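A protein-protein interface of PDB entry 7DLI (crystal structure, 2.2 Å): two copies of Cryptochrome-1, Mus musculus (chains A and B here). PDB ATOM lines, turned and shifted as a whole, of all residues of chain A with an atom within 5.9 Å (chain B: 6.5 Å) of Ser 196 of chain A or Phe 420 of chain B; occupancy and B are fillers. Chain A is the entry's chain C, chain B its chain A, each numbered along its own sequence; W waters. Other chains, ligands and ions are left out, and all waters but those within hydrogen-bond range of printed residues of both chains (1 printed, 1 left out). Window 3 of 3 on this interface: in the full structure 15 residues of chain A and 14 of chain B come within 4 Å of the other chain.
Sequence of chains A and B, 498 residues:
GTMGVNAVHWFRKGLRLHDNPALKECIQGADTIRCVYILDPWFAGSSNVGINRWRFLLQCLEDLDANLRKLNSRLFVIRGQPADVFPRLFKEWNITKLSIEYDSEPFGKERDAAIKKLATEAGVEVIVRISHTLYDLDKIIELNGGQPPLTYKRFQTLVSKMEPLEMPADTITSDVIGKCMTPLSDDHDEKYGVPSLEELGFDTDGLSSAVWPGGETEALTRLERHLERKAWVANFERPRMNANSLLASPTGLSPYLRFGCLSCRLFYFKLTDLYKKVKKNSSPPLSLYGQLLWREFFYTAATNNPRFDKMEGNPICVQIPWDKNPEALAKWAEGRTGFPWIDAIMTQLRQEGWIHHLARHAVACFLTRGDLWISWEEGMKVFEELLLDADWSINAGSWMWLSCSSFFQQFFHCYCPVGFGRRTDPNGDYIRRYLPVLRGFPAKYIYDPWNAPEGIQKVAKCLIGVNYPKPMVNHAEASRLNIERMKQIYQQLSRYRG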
ATOM      1  N   LEU A  58       8.599 -33.312  -7.707  1.00  0.00           N
ATOM      2  CA  LEU A  58       8.791 -32.090  -8.487  1.00  0.00           C
ATOM      3  C   LEU A  58       9.143 -32.410  -9.937  1.00  0.00           C
ATOM      4  O   LEU A  58       8.666 -31.733 -10.861  1.00  0.00           O
ATOM      5  CB  LEU A  58       9.880 -31.211  -7.852  1.00  0.00           C
ATOM      6  CG  LEU A  58       9.572 -30.660  -6.443  1.00  0.00           C
ATOM      7  CD1 LEU A  58      10.677 -29.724  -5.904  1.00  0.00           C
ATOM      8  CD2 LEU A  58       8.217 -29.965  -6.378  1.00  0.00           C
ATOM      9  N   VAL A 194       6.079 -24.771 -11.133  1.00  0.00           N
ATOM     10  CA  VAL A 194       6.557 -25.860 -10.285  1.00  0.00           C
ATOM     11  C   VAL A 194       7.687 -25.334  -9.407  1.00  0.00           C
ATOM     12  O   VAL A 194       8.697 -24.849  -9.935  1.00  0.00           O
ATOM     13  CB  VAL A 194       7.056 -27.052 -11.116  1.00  0.00           C
ATOM     14  CG1 VAL A 194       7.549 -28.160 -10.188  1.00  0.00           C
ATOM     15  CG2 VAL A 194       5.967 -27.554 -12.053  1.00  0.00           C
ATOM     16  N   PRO A 195       7.587 -25.427  -8.087  1.00  0.00           N
ATOM     17  CA  PRO A 195       8.659 -24.900  -7.231  1.00  0.00           C
ATOM     18  C   PRO A 195       9.909 -25.756  -7.345  1.00  0.00           C
ATOM     19  O   PRO A 195       9.856 -26.932  -7.704  1.00  0.00           O
ATOM     20  CB  PRO A 195       8.064 -24.988  -5.826  1.00  0.00           C
ATOM     21  CG  PRO A 195       7.047 -26.107  -5.936  1.00  0.00           C
ATOM     22  CD  PRO A 195       6.482 -26.009  -7.311  1.00  0.00           C
ATOM     23  N   SER A 196      11.047 -25.146  -7.043  1.00  0.00           N
ATOM     24  CA  SER A 196      12.277 -25.907  -6.906  1.00  0.00           C
ATOM     25  C   SER A 196      12.399 -26.435  -5.478  1.00  0.00           C
ATOM     26  O   SER A 196      11.671 -26.022  -4.567  1.00  0.00           O
ATOM     27  CB  SER A 196      13.493 -25.053  -7.264  1.00  0.00           C
ATOM     28  OG  SER A 196      13.781 -24.149  -6.214  1.00  0.00           O
ATOM     29  N   LEU A 197      13.324 -27.380  -5.286  1.00  0.00           N
ATOM     30  CA  LEU A 197      13.582 -27.847  -3.934  1.00  0.00           C
ATOM     31  C   LEU A 197      14.064 -26.711  -3.049  1.00  0.00           C
ATOM     32  O   LEU A 197      13.630 -26.592  -1.897  1.00  0.00           O
ATOM     33  CB  LEU A 197      14.620 -28.965  -3.937  1.00  0.00           C
ATOM     34  CG  LEU A 197      14.215 -30.365  -4.348  1.00  0.00           C
ATOM     35  CD1 LEU A 197      15.468 -31.147  -4.647  1.00  0.00           C
ATOM     36  CD2 LEU A 197      13.396 -31.008  -3.234  1.00  0.00           C
ATOM     37  N   GLU A 198      14.934 -25.844  -3.584  1.00  0.00           N
ATOM     38  CA  GLU A 198      15.473 -24.756  -2.779  1.00  0.00           C
ATOM     39  C   GLU A 198      14.383 -23.756  -2.418  1.00  0.00           C
ATOM     40  O   GLU A 198      14.342 -23.264  -1.292  1.00  0.00           O
ATOM     41  CB  GLU A 198      16.636 -24.075  -3.513  1.00  0.00           C
ATOM     42  N   GLU A 199      13.473 -23.475  -3.355  1.00  0.00           N
ATOM     43  CA  GLU A 199      12.353 -22.581  -3.081  1.00  0.00           C
ATOM     44  C   GLU A 199      11.486 -23.110  -1.943  1.00  0.00           C
ATOM     45  O   GLU A 199      11.003 -22.342  -1.106  1.00  0.00           O
ATOM     46  CB  GLU A 199      11.506 -22.419  -4.348  1.00  0.00           C
ATOM     47  CG  GLU A 199      10.325 -21.472  -4.197  1.00  0.00           C
ATOM     48  CD  GLU A 199       9.640 -21.198  -5.524  1.00  0.00           C
ATOM     49  OE1 GLU A 199       8.506 -20.659  -5.523  1.00  0.00           O
ATOM     50  OE2 GLU A 199      10.246 -21.531  -6.569  1.00  0.00           O
ATOM     51  N   LEU A 200      11.307 -24.417  -1.880  1.00  0.00           N
ATOM     52  CA  LEU A 200      10.529 -25.042  -0.825  1.00  0.00           C
ATOM     53  C   LEU A 200      11.282 -25.130   0.493  1.00  0.00           C
ATOM     54  O   LEU A 200      10.723 -25.656   1.462  1.00  0.00           O
ATOM     55  CB  LEU A 200      10.101 -26.440  -1.258  1.00  0.00           C
ATOM     56  CG  LEU A 200       9.184 -26.452  -2.468  1.00  0.00           C
ATOM     57  CD1 LEU A 200       8.734 -27.880  -2.732  1.00  0.00           C
ATOM     58  CD2 LEU A 200       7.992 -25.526  -2.242  1.00  0.00           C
ATOM     59  N   GLY A 201      12.528 -24.655   0.554  1.00  0.00           N
ATOM     60  CA  GLY A 201      13.256 -24.660   1.805  1.00  0.00           C
ATOM     61  C   GLY A 201      14.133 -25.863   2.080  1.00  0.00           C
ATOM     62  O   GLY A 201      14.639 -25.991   3.197  1.00  0.00           O
ATOM     63  N   TRP B 341      14.751  -8.264  -4.222  1.00  0.00           N
ATOM     64  CA  TRP B 341      15.409  -9.464  -3.701  1.00  0.00           C
ATOM     65  C   TRP B 341      16.896  -9.447  -4.006  1.00  0.00           C
ATOM     66  O   TRP B 341      17.726  -9.691  -3.127  1.00  0.00           O
ATOM     67  CB  TRP B 341      14.753 -10.708  -4.309  1.00  0.00           C
ATOM     68  CG  TRP B 341      15.466 -12.022  -4.173  1.00  0.00           C
ATOM     69  CD1 TRP B 341      16.010 -12.774  -5.186  1.00  0.00           C
ATOM     70  CD2 TRP B 341      15.645 -12.787  -2.972  1.00  0.00           C
ATOM     71  NE1 TRP B 341      16.528 -13.958  -4.680  1.00  0.00           N
ATOM     72  CE2 TRP B 341      16.307 -13.989  -3.329  1.00  0.00           C
ATOM     73  CE3 TRP B 341      15.306 -12.578  -1.637  1.00  0.00           C
ATOM     74  CZ2 TRP B 341      16.651 -14.960  -2.392  1.00  0.00           C
ATOM     75  CZ3 TRP B 341      15.628 -13.563  -0.711  1.00  0.00           C
ATOM     76  CH2 TRP B 341      16.295 -14.731  -1.092  1.00  0.00           C
ATOM     77  N   LEU B 358      22.673 -19.630  -0.773  1.00  0.00           N
ATOM     78  CA  LEU B 358      21.544 -19.528  -1.691  1.00  0.00           C
ATOM     79  C   LEU B 358      21.426 -18.120  -2.266  1.00  0.00           C
ATOM     80  O   LEU B 358      21.128 -17.944  -3.457  1.00  0.00           O
ATOM     81  CB  LEU B 358      20.258 -19.922  -0.962  1.00  0.00           C
ATOM     82  CG  LEU B 358      19.011 -20.192  -1.787  1.00  0.00           C
ATOM     83  CD1 LEU B 358      19.225 -21.455  -2.638  1.00  0.00           C
ATOM     84  CD2 LEU B 358      17.796 -20.363  -0.861  1.00  0.00           C
ATOM     85  N   ALA B 362      21.756 -16.798  -6.244  1.00  0.00           N
ATOM     86  CA  ALA B 362      20.757 -15.931  -6.869  1.00  0.00           C
ATOM     87  C   ALA B 362      21.412 -14.731  -7.559  1.00  0.00           C
ATOM     88  O   ALA B 362      21.136 -14.444  -8.730  1.00  0.00           O
ATOM     89  CB  ALA B 362      19.750 -15.455  -5.821  1.00  0.00           C
ATOM     90  N   TYR B 415      17.306 -18.938 -11.557  1.00  0.00           N
ATOM     91  CA  TYR B 415      16.608 -18.344 -10.419  1.00  0.00           C
ATOM     92  C   TYR B 415      15.767 -17.158 -10.874  1.00  0.00           C
ATOM     93  O   TYR B 415      16.253 -16.286 -11.598  1.00  0.00           O
ATOM     94  CB  TYR B 415      17.615 -17.872  -9.364  1.00  0.00           C
ATOM     95  CG  TYR B 415      18.338 -18.970  -8.610  1.00  0.00           C
ATOM     96  CD1 TYR B 415      19.476 -19.581  -9.143  1.00  0.00           C
ATOM     97  CD2 TYR B 415      17.903 -19.375  -7.352  1.00  0.00           C
ATOM     98  CE1 TYR B 415      20.146 -20.583  -8.450  1.00  0.00           C
ATOM     99  CE2 TYR B 415      18.564 -20.374  -6.654  1.00  0.00           C
ATOM    100  CZ  TYR B 415      19.682 -20.980  -7.205  1.00  0.00           C
ATOM    101  OH  TYR B 415      20.325 -21.975  -6.496  1.00  0.00           O
ATOM    102  N   CYS B 416      14.524 -17.084 -10.426  1.00  0.00           N
ATOM    103  CA  CYS B 416      13.712 -15.917 -10.770  1.00  0.00           C
ATOM    104  C   CYS B 416      14.032 -14.796  -9.783  1.00  0.00           C
ATOM    105  O   CYS B 416      13.951 -15.016  -8.572  1.00  0.00           O
ATOM    106  CB  CYS B 416      12.225 -16.261 -10.754  1.00  0.00           C
ATOM    107  SG  CYS B 416      11.129 -14.794 -10.932  1.00  0.00           S
ATOM    108  N   PRO B 417      14.459 -13.614 -10.246  1.00  0.00           N
ATOM    109  CA  PRO B 417      14.822 -12.530  -9.311  1.00  0.00           C
ATOM    110  C   PRO B 417      13.636 -11.911  -8.580  1.00  0.00           C
ATOM    111  O   PRO B 417      13.864 -11.118  -7.661  1.00  0.00           O
ATOM    112  CB  PRO B 417      15.512 -11.505 -10.216  1.00  0.00           C
ATOM    113  CG  PRO B 417      14.878 -11.726 -11.558  1.00  0.00           C
ATOM    114  CD  PRO B 417      14.633 -13.203 -11.647  1.00  0.00           C
ATOM    115  N   VAL B 418      12.397 -12.259  -8.942  1.00  0.00           N
ATOM    116  CA  VAL B 418      11.197 -11.765  -8.276  1.00  0.00           C
ATOM    117  C   VAL B 418      10.645 -12.793  -7.289  1.00  0.00           C
ATOM    118  O   VAL B 418      10.628 -12.563  -6.078  1.00  0.00           O
ATOM    119  CB  VAL B 418      10.107 -11.431  -9.322  1.00  0.00           C
ATOM    120  CG1 VAL B 418       8.905 -10.755  -8.687  1.00  0.00           C
ATOM    121  CG2 VAL B 418      10.660 -10.585 -10.442  1.00  0.00           C
ATOM    122  N   GLY B 419      10.257 -13.956  -7.797  1.00  0.00           N
ATOM    123  CA  GLY B 419       9.443 -14.884  -7.024  1.00  0.00           C
ATOM    124  C   GLY B 419      10.132 -15.814  -6.044  1.00  0.00           C
ATOM    125  O   GLY B 419       9.497 -16.290  -5.101  1.00  0.00           O
ATOM    126  N   PHE B 420      11.408 -16.126  -6.262  1.00  0.00           N
ATOM    127  CA  PHE B 420      12.038 -17.226  -5.534  1.00  0.00           C
ATOM    128  C   PHE B 420      11.962 -17.062  -4.009  1.00  0.00           C
ATOM    129  O   PHE B 420      11.548 -17.986  -3.298  1.00  0.00           O
ATOM    130  CB  PHE B 420      13.485 -17.358  -5.995  1.00  0.00           C
ATOM    131  CG  PHE B 420      14.236 -18.453  -5.314  1.00  0.00           C
ATOM    132  CD1 PHE B 420      14.087 -19.770  -5.730  1.00  0.00           C
ATOM    133  CD2 PHE B 420      15.107 -18.171  -4.271  1.00  0.00           C
ATOM    134  CE1 PHE B 420      14.791 -20.785  -5.114  1.00  0.00           C
ATOM    135  CE2 PHE B 420      15.808 -19.190  -3.646  1.00  0.00           C
ATOM    136  CZ  PHE B 420      15.646 -20.502  -4.072  1.00  0.00           C
ATOM    137  N   GLY B 421      12.311 -15.883  -3.492  1.00  0.00           N
ATOM    138  CA  GLY B 421      12.342 -15.680  -2.047  1.00  0.00           C
ATOM    139  C   GLY B 421      10.996 -15.783  -1.349  1.00  0.00           C
ATOM    140  O   GLY B 421      10.929 -16.163  -0.172  1.00  0.00           O
ATOM    141  N   ARG B 422       9.910 -15.459  -2.057  1.00  0.00           N
ATOM    142  CA  ARG B 422       8.610 -15.314  -1.418  1.00  0.00           C
ATOM    143  C   ARG B 422       8.140 -16.562  -0.682  1.00  0.00           C
ATOM    144  O   ARG B 422       7.452 -16.438   0.343  1.00  0.00           O
ATOM    145  CB  ARG B 422       7.576 -14.912  -2.464  1.00  0.00           C
ATOM    146  N   ARG B 423       8.502 -17.769  -1.143  1.00  0.00           N
ATOM    147  CA  ARG B 423       7.914 -18.956  -0.515  1.00  0.00           C
ATOM    148  C   ARG B 423       8.388 -19.123   0.924  1.00  0.00           C
ATOM    149  O   ARG B 423       7.588 -19.433   1.818  1.00  0.00           O
ATOM    150  CB  ARG B 423       8.236 -20.213  -1.331  1.00  0.00           C
ATOM    151  N   THR B 424       9.678 -18.914   1.158  1.00  0.00           N
ATOM    152  CA  THR B 424      10.246 -18.964   2.499  1.00  0.00           C
ATOM    153  C   THR B 424      10.060 -17.638   3.253  1.00  0.00           C
ATOM    154  O   THR B 424       9.927 -17.649   4.484  1.00  0.00           O
ATOM    155  CB  THR B 424      11.733 -19.346   2.395  1.00  0.00           C
ATOM    156  OG1 THR B 424      11.861 -20.576   1.659  1.00  0.00           O
ATOM    157  CG2 THR B 424      12.374 -19.504   3.758  1.00  0.00           C
ATOM    158  N   ASP B 425       9.945 -16.506   2.539  1.00  0.00           N
ATOM    159  CA  ASP B 425       9.782 -15.177   3.154  1.00  0.00           C
ATOM    160  C   ASP B 425       8.629 -14.443   2.472  1.00  0.00           C
ATOM    161  O   ASP B 425       8.842 -13.510   1.688  1.00  0.00           O
ATOM    162  CB  ASP B 425      11.091 -14.384   3.052  1.00  0.00           C
ATOM    163  CG  ASP B 425      11.063 -13.056   3.837  1.00  0.00           C
ATOM    164  OD1 ASP B 425      10.061 -12.743   4.505  1.00  0.00           O
ATOM    165  OD2 ASP B 425      12.062 -12.312   3.779  1.00  0.00           O
ATOM    166  N   TYR B 447       8.284  -7.621  -3.518  1.00  0.00           N
ATOM    167  CA  TYR B 447       9.212  -8.248  -4.454  1.00  0.00           C
ATOM    168  C   TYR B 447       9.132  -7.691  -5.870  1.00  0.00           C
ATOM    169  O   TYR B 447      10.023  -7.964  -6.685  1.00  0.00           O
ATOM    170  CB  TYR B 447       8.939  -9.754  -4.534  1.00  0.00           C
ATOM    171  CG  TYR B 447       9.357 -10.529  -3.305  1.00  0.00           C
ATOM    172  CD1 TYR B 447      10.684 -10.937  -3.129  1.00  0.00           C
ATOM    173  CD2 TYR B 447       8.421 -10.879  -2.328  1.00  0.00           C
ATOM    174  CE1 TYR B 447      11.074 -11.659  -2.008  1.00  0.00           C
ATOM    175  CE2 TYR B 447       8.800 -11.603  -1.203  1.00  0.00           C
ATOM    176  CZ  TYR B 447      10.133 -11.986  -1.045  1.00  0.00           C
ATOM    177  OH  TYR B 447      10.501 -12.706   0.073  1.00  0.00           O
HETATM  178  O   HOH W   1       8.117 -18.698  -4.049  1.00  0.00           O
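Water W1 lies within hydrogen-bond range of OE1 of Glu 199 of chain A (2.5 Å), O of Gly 419 of chain B (3.0 Å) and N of Arg 423 of chain B (3.1 Å).
O of Glu 199 of chain A lies within hydrogen-bond range of OG1 of Thr 424 of chain B (3.4 Å).
Among the printed residues, pairs that only touch across the chains: Ser 196 of chain A with Phe 420 of chain B, Glu 198 of chain A with Leu 358 of chain B, Glu 198 of chain A with Phe 420 of chain B, Glu 199 of chain A with Phe 420 of chain B and Glu 199 of chain A with Arg 423 of chain B.
OG of Ser 196 of chain A sits at hydrogen-bond distance from N of Glu 199 of chain A, at 3.0 Å.
The backbone NH of Glu 198 of chain A lies close to the side-chain hydroxyl of Ser 196 of chain A, at 3.3 Å.
Of chain B, only Phe 420 comes within 4 Å of Ser 196 of chain A.
Of chain A, only Ser 196 (3.7 Å), Glu 198 (3.7 Å) and Glu 199 (3.5 Å) come within 4 Å of Phe 420 of chain B.
Of the printed residues of chain A, Thr 424 of chain B touches Glu 199.
Of the printed residues of chain B, Glu 198 of chain A touches Leu 358 (3.8 Å) and Phe 420 (3.7 Å).
Of the printed residues of chain A, Leu 358 of chain B touches Glu 198.
Of the printed residues of chain B, Glu 199 of chain A touches Phe 420, Arg 423 and Thr 424.
Cys 416 of chain B touches none of the printed residues of chain A.
Gly 421 of chain B touches none of the printed residues of chain A.
The nearest printed residue of chain A that does not touch Phe 420 of chain B is Leu 200 of chain A (6.0 Å).
The nearest printed residue of chain B that does not touch Glu 199 of chain A is Gly 419 of chain B (4.5 Å).
No position is printed for both chains.
Printed residues of chain B that touch a printed residue of chain A: Leu 358, Phe 420, Arg 423 and Thr 424.
Hydrophobic or aromatic side chains of chain B that line the printed part of chain A: Leu 358 and Phe 420.
Printed residues of chain A that touch a printed residue of chain B: Ser 196, Glu 198 and Glu 199.
Among the printed residues, no Asp or Glu carboxylate lies within 4 Å of a Lys or Arg side-chain nitrogen of the other chain.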
